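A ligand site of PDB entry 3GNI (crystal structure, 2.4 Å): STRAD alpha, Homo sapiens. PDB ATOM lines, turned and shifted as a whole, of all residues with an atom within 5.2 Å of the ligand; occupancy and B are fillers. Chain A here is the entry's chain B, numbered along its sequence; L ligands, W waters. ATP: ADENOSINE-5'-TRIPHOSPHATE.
Water W5 lies within hydrogen-bond range of an oxygen (O2A) of the ligand, the side-chain hydroxyl of Ser 157 and a ring nitrogen (NE2) of His 158.
Water W3 lies within hydrogen-bond range of O3' of the ligand, OG of Ser 112 and OD1 of Asp 115.
Water W2 lies within hydrogen-bond range of N of Gly 171 (2.7 Å), O1A of the ligand (2.8 Å) and NH2 of Arg 58 (3.5 Å).
Water W4 bridges an oxygen (O2B) of the ligand (2.8 Å) and the guanidinium group of Arg 173 (3.4 Å).
Water W6 lies within hydrogen-bond range of O of Ile 33 (2.7 Å), O2' of the ligand (2.9 Å) and OD1 of Asp 115 (3.1 Å).
Water W1 lies within hydrogen-bond range of OG of Ser 170, O of Ser 157 and O2A of the ligand.
An oxygen (O2') of the ligand sits at hydrogen-bond distance from the side-chain carboxylate of Asp 115 (2.6 Å).
N1 of the ligand sits at hydrogen-bond distance from N of Met 108 (3.1 Å).
NH1 of Arg 58 lies within salt-bridge range of O1A of the ligand, 2.7 Å away.
The side-chain hydroxyl (OG1) of Thr 105 sits at hydrogen-bond distance from a nitrogen (N6) of the ligand, at 3.5 Å.
The guanidinium group (NH2) of Arg 173 is in salt-bridge range of an oxygen (O1B) of the ligand (2.7 Å).
NE2 of His 158 lies within hydrogen-bond range of O2B of the ligand, at 2.7 Å.
The backbone NH (N) of Phe 37 sits at hydrogen-bond distance from an oxygen (O1B) of the ligand.
OG1 of Thr 56 lies close to N1 of the ligand.
A nitrogen (N6) of the ligand lies within hydrogen-bond range of the backbone carbonyl oxygen of Ser 106 (2.9 Å).
An oxygen (O3') of the ligand sits at hydrogen-bond distance from the backbone carbonyl oxygen (O) of Ser 157 (3.0 Å).
CD1 of Ile 33 touches N3 of the ligand (3.4 Å).
Gly 34 touches the ligand.
Lys 35 touches the ligand.
Gly 36 touches the ligand.
CE of Met 41 touches O3A of the ligand, 3.0 Å away.
Val 43 touches the ligand.
OG of Ser 112 touches O3' of the ligand, at 3.9 Å.
Leu 160 touches the ligand (CD1 to N6, 3.6 Å).
Hydrophobic or aromatic side chains within 4 Å of the ligand: Ile 33, Met 41, Val 43, Met 108, His 158 and Leu 160.
Within 4 Å of the ligand: Ile 33, Gly 34, Lys 35, Gly 36, Phe 37, Met 41, Val 43, Thr 56, Arg 58, Thr 105, Ser 106, Met 108, Ser 112, Asp 115, Ser 157, His 158, Leu 160 and Arg 173.
The nearest printed residue that does not touch the ligand is Phe 107 (4.01 Å).
The backbone carbonyl oxygen of His 158 is in hydrogen-bond range of the backbone NH of Ser 170 (2.9 Å).
The backbone NH (N) of Ser 112 sits at hydrogen-bond distance from the side-chain carboxylate (OD2) of Asp 115, at 2.7 Å.
N of Val 43 lies within hydrogen-bond range of O of Gly 34 (3.0 Å).
N of Ile 33 sits at hydrogen-bond distance from O of Val 43 (2.7 Å).
N of Thr 56 sits at hydrogen-bond distance from O of Thr 105.
SD of Met 41 sits close to NH2 of Arg 58 (3.6 Å).
N of Met 41 sits at hydrogen-bond distance from O of Gly 36 (2.9 Å).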
ATOM      1  N   ILE A  33       8.361  14.371  14.016  1.00  0.00           N
ATOM      2  CA  ILE A  33       8.499  15.796  13.697  1.00  0.00           C
ATOM      3  C   ILE A  33       7.191  16.569  13.953  1.00  0.00           C
ATOM      4  O   ILE A  33       7.164  17.808  13.952  1.00  0.00           O
ATOM      5  CB  ILE A  33       9.041  16.026  12.245  1.00  0.00           C
ATOM      6  CG1 ILE A  33       8.101  15.397  11.201  1.00  0.00           C
ATOM      7  CG2 ILE A  33      10.457  15.489  12.131  1.00  0.00           C
ATOM      8  CD1 ILE A  33       8.359  15.820   9.763  1.00  0.00           C
ATOM      9  N   GLY A  34       6.117  15.810  14.182  1.00  0.00           N
ATOM     10  CA  GLY A  34       4.785  16.406  14.345  1.00  0.00           C
ATOM     11  C   GLY A  34       3.712  15.440  14.784  1.00  0.00           C
ATOM     12  O   GLY A  34       3.942  14.240  14.882  1.00  0.00           O
ATOM     13  N   LYS A  35       2.534  15.985  15.026  1.00  0.00           N
ATOM     14  CA  LYS A  35       1.367  15.252  15.519  1.00  0.00           C
ATOM     15  C   LYS A  35       0.100  15.934  14.977  1.00  0.00           C
ATOM     16  O   LYS A  35       0.046  17.162  14.888  1.00  0.00           O
ATOM     17  CB  LYS A  35       1.330  15.279  17.061  1.00  0.00           C
ATOM     18  CG  LYS A  35       0.849  14.007  17.729  1.00  0.00           C
ATOM     19  CD  LYS A  35       2.020  13.114  18.165  1.00  0.00           C
ATOM     20  CE  LYS A  35       1.544  11.907  19.001  1.00  0.00           C
ATOM     21  NZ  LYS A  35       0.819  10.895  18.167  1.00  0.00           N
ATOM     22  N   GLY A  36      -0.899  15.136  14.630  1.00  0.00           N
ATOM     23  CA  GLY A  36      -2.211  15.698  14.282  1.00  0.00           C
ATOM     24  C   GLY A  36      -3.350  14.699  14.247  1.00  0.00           C
ATOM     25  O   GLY A  36      -3.325  13.683  14.959  1.00  0.00           O
ATOM     26  N   PHE A  37      -4.323  14.990  13.376  1.00  0.00           N
ATOM     27  CA  PHE A  37      -5.615  14.301  13.294  1.00  0.00           C
ATOM     28  C   PHE A  37      -6.162  13.867  14.652  1.00  0.00           C
ATOM     29  O   PHE A  37      -6.246  12.683  14.964  1.00  0.00           O
ATOM     30  CB  PHE A  37      -5.577  13.128  12.292  1.00  0.00           C
ATOM     31  CG  PHE A  37      -6.958  12.619  11.898  1.00  0.00           C
ATOM     32  CD1 PHE A  37      -7.967  13.512  11.489  1.00  0.00           C
ATOM     33  CD2 PHE A  37      -7.244  11.254  11.929  1.00  0.00           C
ATOM     34  CE1 PHE A  37      -9.257  13.038  11.133  1.00  0.00           C
ATOM     35  CE2 PHE A  37      -8.511  10.781  11.564  1.00  0.00           C
ATOM     36  CZ  PHE A  37      -9.524  11.682  11.170  1.00  0.00           C
ATOM     37  N   GLU A  38      -6.511  14.857  15.473  1.00  0.00           N
ATOM     38  CA  GLU A  38      -7.093  14.607  16.798  1.00  0.00           C
ATOM     39  C   GLU A  38      -6.193  13.691  17.647  1.00  0.00           C
ATOM     40  O   GLU A  38      -6.679  12.868  18.431  1.00  0.00           O
ATOM     41  CB  GLU A  38      -8.519  14.016  16.651  1.00  0.00           C
ATOM     42  CG  GLU A  38      -9.474  14.822  15.752  1.00  0.00           C
ATOM     43  CD  GLU A  38     -10.153  15.989  16.484  1.00  0.00           C
ATOM     44  OE1 GLU A  38     -10.281  15.955  17.728  1.00  0.00           O
ATOM     45  OE2 GLU A  38     -10.580  16.950  15.795  1.00  0.00           O
ATOM     46  N   MET A  41      -2.647  10.852  14.493  1.00  0.00           N
ATOM     47  CA  MET A  41      -1.587  10.828  13.491  1.00  0.00           C
ATOM     48  C   MET A  41      -0.244  11.232  14.065  1.00  0.00           C
ATOM     49  O   MET A  41      -0.109  12.264  14.729  1.00  0.00           O
ATOM     50  CB  MET A  41      -1.932  11.716  12.300  1.00  0.00           C
ATOM     51  CG  MET A  41      -0.787  11.845  11.305  1.00  0.00           C
ATOM     52  SD  MET A  41      -1.170  12.900   9.901  1.00  0.00           S
ATOM     53  CE  MET A  41      -1.418  14.489  10.677  1.00  0.00           C
ATOM     54  N   VAL A  43       3.509  12.180  12.762  1.00  0.00           N
ATOM     55  CA  VAL A  43       4.276  12.603  11.611  1.00  0.00           C
ATOM     56  C   VAL A  43       5.765  12.351  11.887  1.00  0.00           C
ATOM     57  O   VAL A  43       6.367  12.935  12.784  1.00  0.00           O
ATOM     58  CB  VAL A  43       3.997  14.069  11.193  1.00  0.00           C
ATOM     59  CG1 VAL A  43       4.699  14.392   9.872  1.00  0.00           C
ATOM     60  CG2 VAL A  43       2.481  14.315  11.081  1.00  0.00           C
ATOM     61  N   THR A  56       8.881  12.485   4.629  1.00  0.00           N
ATOM     62  CA  THR A  56       7.947  12.517   5.738  1.00  0.00           C
ATOM     63  C   THR A  56       6.976  11.355   5.625  1.00  0.00           C
ATOM     64  O   THR A  56       6.365  11.157   4.574  1.00  0.00           O
ATOM     65  CB  THR A  56       7.145  13.833   5.712  1.00  0.00           C
ATOM     66  OG1 THR A  56       8.005  14.932   5.985  1.00  0.00           O
ATOM     67  CG2 THR A  56       6.032  13.827   6.716  1.00  0.00           C
ATOM     68  N   ARG A  58       3.495  10.046   7.334  1.00  0.00           N
ATOM     69  CA  ARG A  58       2.309  10.351   8.162  1.00  0.00           C
ATOM     70  C   ARG A  58       1.591   9.046   8.508  1.00  0.00           C
ATOM     71  O   ARG A  58       1.168   8.330   7.606  1.00  0.00           O
ATOM     72  CB  ARG A  58       1.362  11.308   7.420  1.00  0.00           C
ATOM     73  CG  ARG A  58       2.026  12.585   6.908  1.00  0.00           C
ATOM     74  CD  ARG A  58       1.282  13.249   5.743  1.00  0.00           C
ATOM     75  NE  ARG A  58      -0.018  13.793   6.142  1.00  0.00           N
ATOM     76  CZ  ARG A  58      -0.196  14.891   6.888  1.00  0.00           C
ATOM     77  NH1 ARG A  58       0.845  15.586   7.333  1.00  0.00           N
ATOM     78  NH2 ARG A  58      -1.422  15.272   7.211  1.00  0.00           N
ATOM     79  N   VAL A  89       1.876  20.899  -1.440  1.00  0.00           N
ATOM     80  CA  VAL A  89       2.739  19.775  -1.039  1.00  0.00           C
ATOM     81  C   VAL A  89       2.428  18.486  -1.817  1.00  0.00           C
ATOM     82  O   VAL A  89       1.292  18.013  -1.809  1.00  0.00           O
ATOM     83  CB  VAL A  89       2.694  19.533   0.523  1.00  0.00           C
ATOM     84  CG1 VAL A  89       1.304  19.124   0.990  1.00  0.00           C
ATOM     85  CG2 VAL A  89       3.722  18.496   0.940  1.00  0.00           C
ATOM     86  N   THR A 105       5.006  11.985   2.126  1.00  0.00           N
ATOM     87  CA  THR A 105       5.169  13.237   1.383  1.00  0.00           C
ATOM     88  C   THR A 105       6.643  13.648   1.444  1.00  0.00           C
ATOM     89  O   THR A 105       7.417  13.094   2.217  1.00  0.00           O
ATOM     90  CB  THR A 105       4.282  14.377   1.957  1.00  0.00           C
ATOM     91  OG1 THR A 105       4.644  14.625   3.314  1.00  0.00           O
ATOM     92  CG2 THR A 105       2.802  13.985   1.918  1.00  0.00           C
ATOM     93  N   SER A 106       7.041  14.603   0.595  1.00  0.00           N
ATOM     94  CA  SER A 106       8.390  15.156   0.671  1.00  0.00           C
ATOM     95  C   SER A 106       8.612  15.923   1.985  1.00  0.00           C
ATOM     96  O   SER A 106       7.677  16.512   2.544  1.00  0.00           O
ATOM     97  CB  SER A 106       8.690  16.027  -0.546  1.00  0.00           C
ATOM     98  OG  SER A 106      10.093  16.028  -0.780  1.00  0.00           O
ATOM     99  N   PHE A 107       9.836  15.873   2.496  1.00  0.00           N
ATOM    100  CA  PHE A 107      10.182  16.466   3.779  1.00  0.00           C
ATOM    101  C   PHE A 107      10.581  17.931   3.597  1.00  0.00           C
ATOM    102  O   PHE A 107      11.463  18.244   2.794  1.00  0.00           O
ATOM    103  CB  PHE A 107      11.317  15.669   4.430  1.00  0.00           C
ATOM    104  CG  PHE A 107      11.908  16.325   5.667  1.00  0.00           C
ATOM    105  CD1 PHE A 107      11.150  16.486   6.825  1.00  0.00           C
ATOM    106  CD2 PHE A 107      13.232  16.749   5.664  1.00  0.00           C
ATOM    107  CE1 PHE A 107      11.686  17.085   7.972  1.00  0.00           C
ATOM    108  CE2 PHE A 107      13.804  17.351   6.804  1.00  0.00           C
ATOM    109  CZ  PHE A 107      13.029  17.523   7.966  1.00  0.00           C
ATOM    110  N   MET A 108       9.912  18.823   4.336  1.00  0.00           N
ATOM    111  CA  MET A 108      10.200  20.260   4.275  1.00  0.00           C
ATOM    112  C   MET A 108      11.038  20.647   5.489  1.00  0.00           C
ATOM    113  O   MET A 108      10.517  20.722   6.604  1.00  0.00           O
ATOM    114  CB  MET A 108       8.906  21.080   4.195  1.00  0.00           C
ATOM    115  CG  MET A 108       7.864  20.532   3.217  1.00  0.00           C
ATOM    116  SD  MET A 108       8.484  20.492   1.532  1.00  0.00           S
ATOM    117  CE  MET A 108       7.231  19.515   0.709  1.00  0.00           C
ATOM    118  N   GLY A 111      10.305  22.934   8.377  1.00  0.00           N
ATOM    119  CA  GLY A 111       9.023  22.640   9.003  1.00  0.00           C
ATOM    120  C   GLY A 111       7.956  23.628   8.603  1.00  0.00           C
ATOM    121  O   GLY A 111       8.025  24.207   7.497  1.00  0.00           O
ATOM    122  N   SER A 112       6.968  23.810   9.479  1.00  0.00           N
ATOM    123  CA  SER A 112       5.879  24.767   9.230  1.00  0.00           C
ATOM    124  C   SER A 112       6.182  26.187   9.770  1.00  0.00           C
ATOM    125  O   SER A 112       7.064  26.353  10.617  1.00  0.00           O
ATOM    126  CB  SER A 112       4.554  24.235   9.798  1.00  0.00           C
ATOM    127  OG  SER A 112       4.385  24.592  11.159  1.00  0.00           O
ATOM    128  N   ASP A 115       6.001  26.025  13.456  1.00  0.00           N
ATOM    129  CA  ASP A 115       7.278  25.500  13.978  1.00  0.00           C
ATOM    130  C   ASP A 115       8.327  26.584  14.126  1.00  0.00           C
ATOM    131  O   ASP A 115       8.995  26.681  15.176  1.00  0.00           O
ATOM    132  CB  ASP A 115       7.826  24.405  13.055  1.00  0.00           C
ATOM    133  CG  ASP A 115       6.921  23.181  12.985  1.00  0.00           C
ATOM    134  OD1 ASP A 115       6.272  22.855  14.006  1.00  0.00           O
ATOM    135  OD2 ASP A 115       6.852  22.535  11.905  1.00  0.00           O
ATOM    136  N   LYS A 155      -3.805  27.996   7.905  1.00  0.00           N
ATOM    137  CA  LYS A 155      -3.213  28.410   9.177  1.00  0.00           C
ATOM    138  C   LYS A 155      -1.697  28.185   9.064  1.00  0.00           C
ATOM    139  O   LYS A 155      -1.244  27.518   8.125  1.00  0.00           O
ATOM    140  CB  LYS A 155      -3.804  27.609  10.344  1.00  0.00           C
ATOM    141  CG  LYS A 155      -3.802  26.075  10.148  1.00  0.00           C
ATOM    142  CD  LYS A 155      -4.573  25.336  11.251  1.00  0.00           C
ATOM    143  CE  LYS A 155      -3.951  25.570  12.625  1.00  0.00           C
ATOM    144  NZ  LYS A 155      -4.371  24.559  13.646  1.00  0.00           N
ATOM    145  N   SER A 157       0.433  26.369  10.688  1.00  0.00           N
ATOM    146  CA  SER A 157       0.879  24.981  10.779  1.00  0.00           C
ATOM    147  C   SER A 157       0.574  24.178   9.516  1.00  0.00           C
ATOM    148  O   SER A 157       1.041  23.046   9.356  1.00  0.00           O
ATOM    149  CB  SER A 157       0.302  24.289  12.026  1.00  0.00           C
ATOM    150  OG  SER A 157      -1.084  24.037  11.909  1.00  0.00           O
ATOM    151  N   HIS A 158      -0.189  24.780   8.600  1.00  0.00           N
ATOM    152  CA  HIS A 158      -0.452  24.197   7.285  1.00  0.00           C
ATOM    153  C   HIS A 158       0.297  24.907   6.165  1.00  0.00           C
ATOM    154  O   HIS A 158      -0.143  24.902   5.015  1.00  0.00           O
ATOM    155  CB  HIS A 158      -1.960  24.160   6.984  1.00  0.00           C
ATOM    156  CG  HIS A 158      -2.696  23.075   7.710  1.00  0.00           C
ATOM    157  ND1 HIS A 158      -4.061  23.108   7.910  1.00  0.00           N
ATOM    158  CD2 HIS A 158      -2.248  21.973   8.352  1.00  0.00           C
ATOM    159  CE1 HIS A 158      -4.423  22.037   8.601  1.00  0.00           C
ATOM    160  NE2 HIS A 158      -3.343  21.339   8.891  1.00  0.00           N
ATOM    161  N   LEU A 160       4.329  24.979   4.860  1.00  0.00           N
ATOM    162  CA  LEU A 160       5.609  24.297   5.031  1.00  0.00           C
ATOM    163  C   LEU A 160       6.678  24.949   4.161  1.00  0.00           C
ATOM    164  O   LEU A 160       6.401  25.418   3.054  1.00  0.00           O
ATOM    165  CB  LEU A 160       5.476  22.807   4.697  1.00  0.00           C
ATOM    166  CG  LEU A 160       4.396  22.026   5.444  1.00  0.00           C
ATOM    167  CD1 LEU A 160       4.191  20.648   4.799  1.00  0.00           C
ATOM    168  CD2 LEU A 160       4.729  21.879   6.923  1.00  0.00           C
ATOM    169  N   SER A 170      -0.216  22.928   2.919  1.00  0.00           N
ATOM    170  CA  SER A 170      -0.613  21.560   3.264  1.00  0.00           C
ATOM    171  C   SER A 170      -2.067  21.549   3.725  1.00  0.00           C
ATOM    172  O   SER A 170      -2.854  22.420   3.349  1.00  0.00           O
ATOM    173  CB  SER A 170       0.335  20.973   4.319  1.00  0.00           C
ATOM    174  OG  SER A 170       0.345  21.757   5.498  1.00  0.00           O
ATOM    175  N   GLY A 171      -2.443  20.553   4.521  1.00  0.00           N
ATOM    176  CA  GLY A 171      -3.775  20.543   5.152  1.00  0.00           C
ATOM    177  C   GLY A 171      -4.941  20.215   4.240  1.00  0.00           C
ATOM    178  O   GLY A 171      -6.080  20.656   4.467  1.00  0.00           O
ATOM    179  N   ARG A 173      -6.616  17.541   3.884  1.00  0.00           N
ATOM    180  CA  ARG A 173      -7.658  16.724   4.526  1.00  0.00           C
ATOM    181  C   ARG A 173      -9.015  17.430   4.698  1.00  0.00           C
ATOM    182  O   ARG A 173     -10.073  16.791   4.607  1.00  0.00           O
ATOM    183  CB  ARG A 173      -7.177  16.239   5.892  1.00  0.00           C
ATOM    184  CG  ARG A 173      -7.976  15.106   6.475  1.00  0.00           C
ATOM    185  CD  ARG A 173      -7.834  15.046   7.980  1.00  0.00           C
ATOM    186  NE  ARG A 173      -6.468  14.768   8.366  1.00  0.00           N
ATOM    187  CZ  ARG A 173      -5.774  15.484   9.250  1.00  0.00           C
ATOM    188  NH1 ARG A 173      -6.321  16.513   9.879  1.00  0.00           N
ATOM    189  NH2 ARG A 173      -4.529  15.136   9.509  1.00  0.00           N
ATOM    190  N   VAL A 198      -9.218  24.396  14.623  1.00  0.00           N
ATOM    191  CA  VAL A 198      -9.125  25.249  13.445  1.00  0.00           C
ATOM    192  C   VAL A 198     -10.131  26.394  13.525  1.00  0.00           C
ATOM    193  O   VAL A 198     -10.103  27.322  12.706  1.00  0.00           O
ATOM    194  CB  VAL A 198      -9.325  24.469  12.103  1.00  0.00           C
ATOM    195  CG1 VAL A 198      -8.886  25.306  10.905  1.00  0.00           C
ATOM    196  CG2 VAL A 198      -8.550  23.154  12.116  1.00  0.00           C
HETATM  197  PG  ATP L   1      -3.887  19.487  13.336  1.00  0.00           P
HETATM  198  O1G ATP L   1      -3.105  19.934  14.565  1.00  0.00           O
HETATM  199  O2G ATP L   1      -4.814  18.327  13.634  1.00  0.00           O
HETATM  200  O3G ATP L   1      -4.534  20.599  12.533  1.00  0.00           O
HETATM  201  PB  ATP L   1      -2.902  18.010  11.078  1.00  0.00           P
HETATM  202  O1B ATP L   1      -3.689  16.803  11.490  1.00  0.00           O
HETATM  203  O2B ATP L   1      -3.365  18.836   9.911  1.00  0.00           O
HETATM  204  O3B ATP L   1      -2.702  18.964  12.362  1.00  0.00           O
HETATM  205  PA  ATP L   1      -0.334  18.305   9.800  1.00  0.00           P
HETATM  206  O1A ATP L   1      -0.409  17.699   8.424  1.00  0.00           O
HETATM  207  O2A ATP L   1      -0.464  19.796   9.928  1.00  0.00           O
HETATM  208  O3A ATP L   1      -1.387  17.534  10.757  1.00  0.00           O
HETATM  209  O5' ATP L   1       1.025  17.817  10.484  1.00  0.00           O
HETATM  210  C5' ATP L   1       1.329  18.248  11.815  1.00  0.00           C
HETATM  211  C4' ATP L   1       2.695  18.910  11.824  1.00  0.00           C
HETATM  212  O4' ATP L   1       3.671  17.965  11.369  1.00  0.00           O
HETATM  213  C3' ATP L   1       2.842  20.077  10.868  1.00  0.00           C
HETATM  214  O3' ATP L   1       2.351  21.312  11.382  1.00  0.00           O
HETATM  215  C2' ATP L   1       4.340  20.119  10.675  1.00  0.00           C
HETATM  216  O2' ATP L   1       4.986  20.728  11.804  1.00  0.00           O
HETATM  217  C1' ATP L   1       4.694  18.633  10.627  1.00  0.00           C
HETATM  218  N9  ATP L   1       4.699  18.250   9.192  1.00  0.00           N
HETATM  219  C8  ATP L   1       3.660  17.774   8.465  1.00  0.00           C
HETATM  220  N7  ATP L   1       4.021  17.562   7.175  1.00  0.00           N
HETATM  221  C5  ATP L   1       5.330  17.897   7.034  1.00  0.00           C
HETATM  222  C6  ATP L   1       6.328  17.904   5.940  1.00  0.00           C
HETATM  223  N6  ATP L   1       6.029  17.514   4.675  1.00  0.00           N
HETATM  224  N1  ATP L   1       7.576  18.330   6.246  1.00  0.00           N
HETATM  225  C2  ATP L   1       7.906  18.742   7.480  1.00  0.00           C
HETATM  226  N3  ATP L   1       7.058  18.762   8.523  1.00  0.00           N
HETATM  227  C4  ATP L   1       5.767  18.351   8.367  1.00  0.00           C
HETATM  228  O   HOH W   1       1.289  20.868   7.762  1.00  0.00           O
HETATM  229  O   HOH W   2      -1.505  18.511   6.016  1.00  0.00           O
HETATM  230  O   HOH W   3       3.443  23.024  13.241  1.00  0.00           O
HETATM  231  O   HOH W   4      -4.542  18.064   7.452  1.00  0.00           O
HETATM  232  O   HOH W   5      -1.246  21.398  11.661  1.00  0.00           O
HETATM  233  O   HOH W   6       5.515  19.898  14.576  1.00  0.00           O
